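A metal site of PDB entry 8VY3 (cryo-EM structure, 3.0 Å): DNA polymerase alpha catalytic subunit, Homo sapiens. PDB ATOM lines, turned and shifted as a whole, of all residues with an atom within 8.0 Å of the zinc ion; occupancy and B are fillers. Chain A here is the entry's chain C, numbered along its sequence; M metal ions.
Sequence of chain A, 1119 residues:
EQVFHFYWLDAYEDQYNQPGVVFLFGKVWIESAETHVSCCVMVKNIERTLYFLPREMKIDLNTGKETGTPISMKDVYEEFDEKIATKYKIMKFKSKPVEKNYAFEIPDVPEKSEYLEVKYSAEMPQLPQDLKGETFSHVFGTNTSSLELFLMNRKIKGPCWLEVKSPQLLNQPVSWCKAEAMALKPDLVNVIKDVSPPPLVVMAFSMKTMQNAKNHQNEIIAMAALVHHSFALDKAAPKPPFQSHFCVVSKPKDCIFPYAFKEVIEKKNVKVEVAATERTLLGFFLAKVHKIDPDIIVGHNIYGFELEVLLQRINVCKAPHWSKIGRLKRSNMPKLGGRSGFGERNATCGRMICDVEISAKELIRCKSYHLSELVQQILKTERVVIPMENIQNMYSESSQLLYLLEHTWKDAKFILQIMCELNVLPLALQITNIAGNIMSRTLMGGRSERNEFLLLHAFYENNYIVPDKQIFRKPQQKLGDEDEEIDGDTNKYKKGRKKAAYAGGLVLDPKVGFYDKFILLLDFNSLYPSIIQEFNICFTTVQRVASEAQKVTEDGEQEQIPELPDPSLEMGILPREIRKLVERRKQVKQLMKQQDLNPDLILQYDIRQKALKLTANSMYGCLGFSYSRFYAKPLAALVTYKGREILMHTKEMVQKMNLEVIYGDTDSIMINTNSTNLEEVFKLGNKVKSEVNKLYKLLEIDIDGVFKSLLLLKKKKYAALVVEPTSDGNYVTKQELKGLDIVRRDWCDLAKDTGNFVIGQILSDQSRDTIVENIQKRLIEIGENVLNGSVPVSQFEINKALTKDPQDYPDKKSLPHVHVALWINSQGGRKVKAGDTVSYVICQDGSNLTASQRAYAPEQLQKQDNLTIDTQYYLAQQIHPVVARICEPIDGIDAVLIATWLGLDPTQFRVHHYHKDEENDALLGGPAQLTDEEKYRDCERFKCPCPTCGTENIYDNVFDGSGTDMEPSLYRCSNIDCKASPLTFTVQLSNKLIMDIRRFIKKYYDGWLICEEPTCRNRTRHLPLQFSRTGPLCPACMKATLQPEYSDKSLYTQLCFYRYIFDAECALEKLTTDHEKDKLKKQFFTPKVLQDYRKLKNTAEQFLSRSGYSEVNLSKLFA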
ATOM      1  N   PRO A 945     -20.285  30.572   7.316  1.00  0.00           N
ATOM      2  CA  PRO A 945     -20.414  29.987   5.981  1.00  0.00           C
ATOM      3  C   PRO A 945     -19.081  29.875   5.259  1.00  0.00           C
ATOM      4  O   PRO A 945     -18.169  30.675   5.455  1.00  0.00           O
ATOM      5  CB  PRO A 945     -21.352  30.959   5.265  1.00  0.00           C
ATOM      6  CG  PRO A 945     -21.087  32.264   5.929  1.00  0.00           C
ATOM      7  CD  PRO A 945     -20.832  31.938   7.373  1.00  0.00           C
ATOM      8  N   CYS A 946     -18.988  28.857   4.413  1.00  0.00           N
ATOM      9  CA  CYS A 946     -17.781  28.629   3.626  1.00  0.00           C
ATOM     10  C   CYS A 946     -17.662  29.693   2.540  1.00  0.00           C
ATOM     11  O   CYS A 946     -18.631  29.938   1.813  1.00  0.00           O
ATOM     12  CB  CYS A 946     -17.829  27.229   2.999  1.00  0.00           C
ATOM     13  SG  CYS A 946     -16.302  26.698   2.183  1.00  0.00           S
ATOM     14  N   PRO A 947     -16.509  30.359   2.403  1.00  0.00           N
ATOM     15  CA  PRO A 947     -16.369  31.421   1.404  1.00  0.00           C
ATOM     16  C   PRO A 947     -16.546  30.941  -0.023  1.00  0.00           C
ATOM     17  O   PRO A 947     -16.852  31.728  -0.922  1.00  0.00           O
ATOM     18  CB  PRO A 947     -14.957  31.954   1.651  1.00  0.00           C
ATOM     19  CG  PRO A 947     -14.643  31.566   3.057  1.00  0.00           C
ATOM     20  CD  PRO A 947     -15.293  30.226   3.219  1.00  0.00           C
ATOM     21  N   THR A 948     -16.341  29.645  -0.261  1.00  0.00           N
ATOM     22  CA  THR A 948     -16.413  29.066  -1.597  1.00  0.00           C
ATOM     23  C   THR A 948     -17.789  28.504  -1.926  1.00  0.00           C
ATOM     24  O   THR A 948     -18.427  28.947  -2.893  1.00  0.00           O
ATOM     25  CB  THR A 948     -15.350  27.978  -1.761  1.00  0.00           C
ATOM     26  OG1 THR A 948     -14.119  28.409  -1.176  1.00  0.00           O
ATOM     27  CG2 THR A 948     -15.117  27.682  -3.236  1.00  0.00           C
ATOM     28  N   CYS A 949     -18.266  27.530  -1.163  1.00  0.00           N
ATOM     29  CA  CYS A 949     -19.542  26.883  -1.462  1.00  0.00           C
ATOM     30  C   CYS A 949     -20.731  27.542  -0.786  1.00  0.00           C
ATOM     31  O   CYS A 949     -21.847  27.435  -1.290  1.00  0.00           O
ATOM     32  CB  CYS A 949     -19.482  25.403  -1.068  1.00  0.00           C
ATOM     33  SG  CYS A 949     -19.297  25.084   0.698  1.00  0.00           S
ATOM     34  N   GLY A 950     -20.524  28.219   0.350  1.00  0.00           N
ATOM     35  CA  GLY A 950     -21.589  28.910   1.052  1.00  0.00           C
ATOM     36  C   GLY A 950     -22.320  28.071   2.078  1.00  0.00           C
ATOM     37  O   GLY A 950     -23.188  28.598   2.777  1.00  0.00           O
ATOM     38  N   THR A 951     -21.993  26.781   2.180  1.00  0.00           N
ATOM     39  CA  THR A 951     -22.660  25.921   3.145  1.00  0.00           C
ATOM     40  C   THR A 951     -22.280  26.323   4.561  1.00  0.00           C
ATOM     41  O   THR A 951     -21.108  26.581   4.868  1.00  0.00           O
ATOM     42  CB  THR A 951     -22.274  24.457   2.888  1.00  0.00           C
ATOM     43  OG1 THR A 951     -22.749  24.066   1.598  1.00  0.00           O
ATOM     44  CG2 THR A 951     -22.894  23.552   3.940  1.00  0.00           C
ATOM     45  N   GLU A 952     -23.281  26.367   5.437  1.00  0.00           N
ATOM     46  CA  GLU A 952     -23.059  26.744   6.818  1.00  0.00           C
ATOM     47  C   GLU A 952     -22.298  25.654   7.556  1.00  0.00           C
ATOM     48  O   GLU A 952     -22.585  24.469   7.396  1.00  0.00           O
ATOM     49  CB  GLU A 952     -24.399  27.011   7.510  1.00  0.00           C
ATOM     50  CG  GLU A 952     -24.417  28.253   8.393  1.00  0.00           C
ATOM     51  CD  GLU A 952     -25.452  28.163   9.490  1.00  0.00           C
ATOM     52  OE1 GLU A 952     -25.514  29.083  10.328  1.00  0.00           O
ATOM     53  OE2 GLU A 952     -26.212  27.162   9.512  1.00  0.00           O
ATOM     54  N   ASN A 953     -21.316  26.063   8.360  1.00  0.00           N
ATOM     55  CA  ASN A 953     -20.487  25.139   9.123  1.00  0.00           C
ATOM     56  C   ASN A 953     -20.754  25.319  10.616  1.00  0.00           C
ATOM     57  O   ASN A 953     -20.951  26.442  11.089  1.00  0.00           O
ATOM     58  CB  ASN A 953     -19.003  25.367   8.836  1.00  0.00           C
ATOM     59  CG  ASN A 953     -18.530  24.607   7.613  1.00  0.00           C
ATOM     60  OD1 ASN A 953     -18.673  25.065   6.488  1.00  0.00           O
ATOM     61  ND2 ASN A 953     -17.945  23.436   7.844  1.00  0.00           N
ATOM     62  N   ARG A 972     -11.479  19.996   7.046  1.00  0.00           N
ATOM     63  CA  ARG A 972     -12.187  19.906   5.783  1.00  0.00           C
ATOM     64  C   ARG A 972     -13.580  20.512   5.922  1.00  0.00           C
ATOM     65  O   ARG A 972     -14.179  20.498   6.997  1.00  0.00           O
ATOM     66  CB  ARG A 972     -12.296  18.457   5.307  1.00  0.00           C
ATOM     67  CG  ARG A 972     -13.363  17.628   6.004  1.00  0.00           C
ATOM     68  CD  ARG A 972     -13.878  16.512   5.108  1.00  0.00           C
ATOM     69  NE  ARG A 972     -12.814  15.750   4.456  1.00  0.00           N
ATOM     70  CZ  ARG A 972     -11.871  15.058   5.079  1.00  0.00           C
ATOM     71  NH1 ARG A 972     -11.846  14.951   6.392  1.00  0.00           N
ATOM     72  NH2 ARG A 972     -10.942  14.441   4.360  1.00  0.00           N
ATOM     73  N   CYS A 973     -14.085  21.049   4.808  1.00  0.00           N
ATOM     74  CA  CYS A 973     -15.396  21.676   4.807  1.00  0.00           C
ATOM     75  C   CYS A 973     -16.483  20.620   4.980  1.00  0.00           C
ATOM     76  O   CYS A 973     -16.324  19.474   4.565  1.00  0.00           O
ATOM     77  CB  CYS A 973     -15.602  22.459   3.511  1.00  0.00           C
ATOM     78  SG  CYS A 973     -17.286  23.057   3.216  1.00  0.00           S
ATOM     79  N   SER A 974     -17.606  21.014   5.602  1.00  0.00           N
ATOM     80  CA  SER A 974     -18.683  20.069   5.853  1.00  0.00           C
ATOM     81  C   SER A 974     -19.360  19.595   4.575  1.00  0.00           C
ATOM     82  O   SER A 974     -19.903  18.487   4.545  1.00  0.00           O
ATOM     83  CB  SER A 974     -19.725  20.700   6.781  1.00  0.00           C
ATOM     84  OG  SER A 974     -20.493  21.670   6.093  1.00  0.00           O
ATOM     85  N   ASN A 975     -19.347  20.411   3.527  1.00  0.00           N
ATOM     86  CA  ASN A 975     -19.940  20.024   2.253  1.00  0.00           C
ATOM     87  C   ASN A 975     -19.072  18.957   1.597  1.00  0.00           C
ATOM     88  O   ASN A 975     -17.850  19.120   1.488  1.00  0.00           O
ATOM     89  CB  ASN A 975     -20.085  21.244   1.337  1.00  0.00           C
ATOM     90  CG  ASN A 975     -20.815  20.916   0.057  1.00  0.00           C
ATOM     91  OD1 ASN A 975     -21.904  20.337   0.076  1.00  0.00           O
ATOM     92  ND2 ASN A 975     -20.224  21.296  -1.069  1.00  0.00           N
ATOM     93  N   ILE A 976     -19.699  17.872   1.148  1.00  0.00           N
ATOM     94  CA  ILE A 976     -18.954  16.775   0.540  1.00  0.00           C
ATOM     95  C   ILE A 976     -18.361  17.211  -0.789  1.00  0.00           C
ATOM     96  O   ILE A 976     -17.220  16.863  -1.123  1.00  0.00           O
ATOM     97  CB  ILE A 976     -19.865  15.542   0.371  1.00  0.00           C
ATOM     98  CG1 ILE A 976     -20.673  15.303   1.637  1.00  0.00           C
ATOM     99  CG2 ILE A 976     -19.032  14.316   0.023  1.00  0.00           C
ATOM    100  CD1 ILE A 976     -21.674  14.170   1.522  1.00  0.00           C
ATOM    101  N   ASP A 977     -19.117  17.990  -1.558  1.00  0.00           N
ATOM    102  CA  ASP A 977     -18.661  18.464  -2.861  1.00  0.00           C
ATOM    103  C   ASP A 977     -17.572  19.527  -2.754  1.00  0.00           C
ATOM    104  O   ASP A 977     -16.872  19.767  -3.749  1.00  0.00           O
ATOM    105  CB  ASP A 977     -19.835  19.027  -3.657  1.00  0.00           C
ATOM    106  CG  ASP A 977     -20.594  17.956  -4.408  1.00  0.00           C
ATOM    107  OD1 ASP A 977     -19.978  17.272  -5.252  1.00  0.00           O
ATOM    108  OD2 ASP A 977     -21.805  17.797  -4.163  1.00  0.00           O
ATOM    109  N   CYS A 978     -17.401  20.157  -1.595  1.00  0.00           N
ATOM    110  CA  CYS A 978     -16.441  21.236  -1.445  1.00  0.00           C
ATOM    111  C   CYS A 978     -15.087  20.680  -0.981  1.00  0.00           C
ATOM    112  O   CYS A 978     -15.020  19.896  -0.029  1.00  0.00           O
ATOM    113  CB  CYS A 978     -16.941  22.272  -0.443  1.00  0.00           C
ATOM    114  SG  CYS A 978     -15.878  23.722  -0.237  1.00  0.00           S
ATOM    115  N   LYS A 979     -14.027  21.100  -1.668  1.00  0.00           N
ATOM    116  CA  LYS A 979     -12.676  20.678  -1.325  1.00  0.00           C
ATOM    117  C   LYS A 979     -11.848  21.810  -0.717  1.00  0.00           C
ATOM    118  O   LYS A 979     -10.612  21.712  -0.686  1.00  0.00           O
ATOM    119  CB  LYS A 979     -11.959  20.114  -2.559  1.00  0.00           C
ATOM    120  CG  LYS A 979     -10.993  18.981  -2.265  1.00  0.00           C
ATOM    121  CD  LYS A 979     -11.706  17.719  -1.781  1.00  0.00           C
ATOM    122  CE  LYS A 979     -12.925  17.388  -2.634  1.00  0.00           C
ATOM    123  NZ  LYS A 979     -13.541  16.103  -2.224  1.00  0.00           N
ATOM    124  N   ALA A 980     -12.493  22.866  -0.239  1.00  0.00           N
ATOM    125  CA  ALA A 980     -11.780  23.965   0.402  1.00  0.00           C
ATOM    126  C   ALA A 980     -11.623  23.705   1.891  1.00  0.00           C
ATOM    127  O   ALA A 980     -12.569  23.297   2.576  1.00  0.00           O
ATOM    128  CB  ALA A 980     -12.503  25.285   0.172  1.00  0.00           C
ATOM    129  N   SER A 981     -10.413  23.940   2.396  1.00  0.00           N
ATOM    130  CA  SER A 981     -10.110  23.709   3.795  1.00  0.00           C
ATOM    131  C   SER A 981     -10.416  24.966   4.591  1.00  0.00           C
ATOM    132  O   SER A 981      -9.896  26.046   4.250  1.00  0.00           O
ATOM    133  CB  SER A 981      -8.648  23.320   3.965  1.00  0.00           C
ATOM    134  OG  SER A 981      -8.339  23.056   5.327  1.00  0.00           O
ATOM    135  N   PRO A 982     -11.250  24.899   5.639  1.00  0.00           N
ATOM    136  CA  PRO A 982     -11.501  26.098   6.453  1.00  0.00           C
ATOM    137  C   PRO A 982     -10.256  26.640   7.125  1.00  0.00           C
ATOM    138  O   PRO A 982     -10.226  27.812   7.498  1.00  0.00           O
ATOM    139  CB  PRO A 982     -12.523  25.596   7.476  1.00  0.00           C
ATOM    140  CG  PRO A 982     -13.217  24.474   6.783  1.00  0.00           C
ATOM    141  CD  PRO A 982     -12.122  23.779   6.024  1.00  0.00           C
ATOM    142  N   PHE A 985      -8.896  29.668   5.349  1.00  0.00           N
ATOM    143  CA  PHE A 985      -9.662  30.891   5.573  1.00  0.00           C
ATOM    144  C   PHE A 985      -9.713  31.240   7.064  1.00  0.00           C
ATOM    145  O   PHE A 985     -10.783  31.346   7.658  1.00  0.00           O
ATOM    146  CB  PHE A 985     -11.072  30.731   5.013  1.00  0.00           C
ATOM    147  CG  PHE A 985     -11.098  30.492   3.527  1.00  0.00           C
ATOM    148  CD1 PHE A 985     -11.733  29.377   3.005  1.00  0.00           C
ATOM    149  CD2 PHE A 985     -10.488  31.379   2.652  1.00  0.00           C
ATOM    150  CE1 PHE A 985     -11.764  29.160   1.641  1.00  0.00           C
ATOM    151  CE2 PHE A 985     -10.519  31.163   1.288  1.00  0.00           C
ATOM    152  CZ  PHE A 985     -11.151  30.055   0.786  1.00  0.00           C
HETATM  153 ZN    ZN M   1     -17.157  24.629   1.496  1.00  0.00          ZN
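The side-chain amide nitrogen (ND2) of Asn 975 lies close to the backbone NH (N) of Cys 978 (3.1 Å).
SG of Cys 978 sits close to N of Ala 980, at 3.5 Å.
O of Thr 951 lies within hydrogen-bond range of N of Cys 946, 3.1 Å away.
SG of Cys 949 sits close to N of Thr 951 (3.5 Å).
SG of Cys 973 lies close to N of Asn 975, 3.4 Å away.
Four residues have an atom within 4 Å of the zinc ion: Cys 946, Cys 949, Cys 973 and Cys 978.
The zinc ion is bound by SG of Cys 949, SG of Cys 973, SG of Cys 978 and SG of Cys 946.
The zinc ion has four donor atoms within binding distance.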
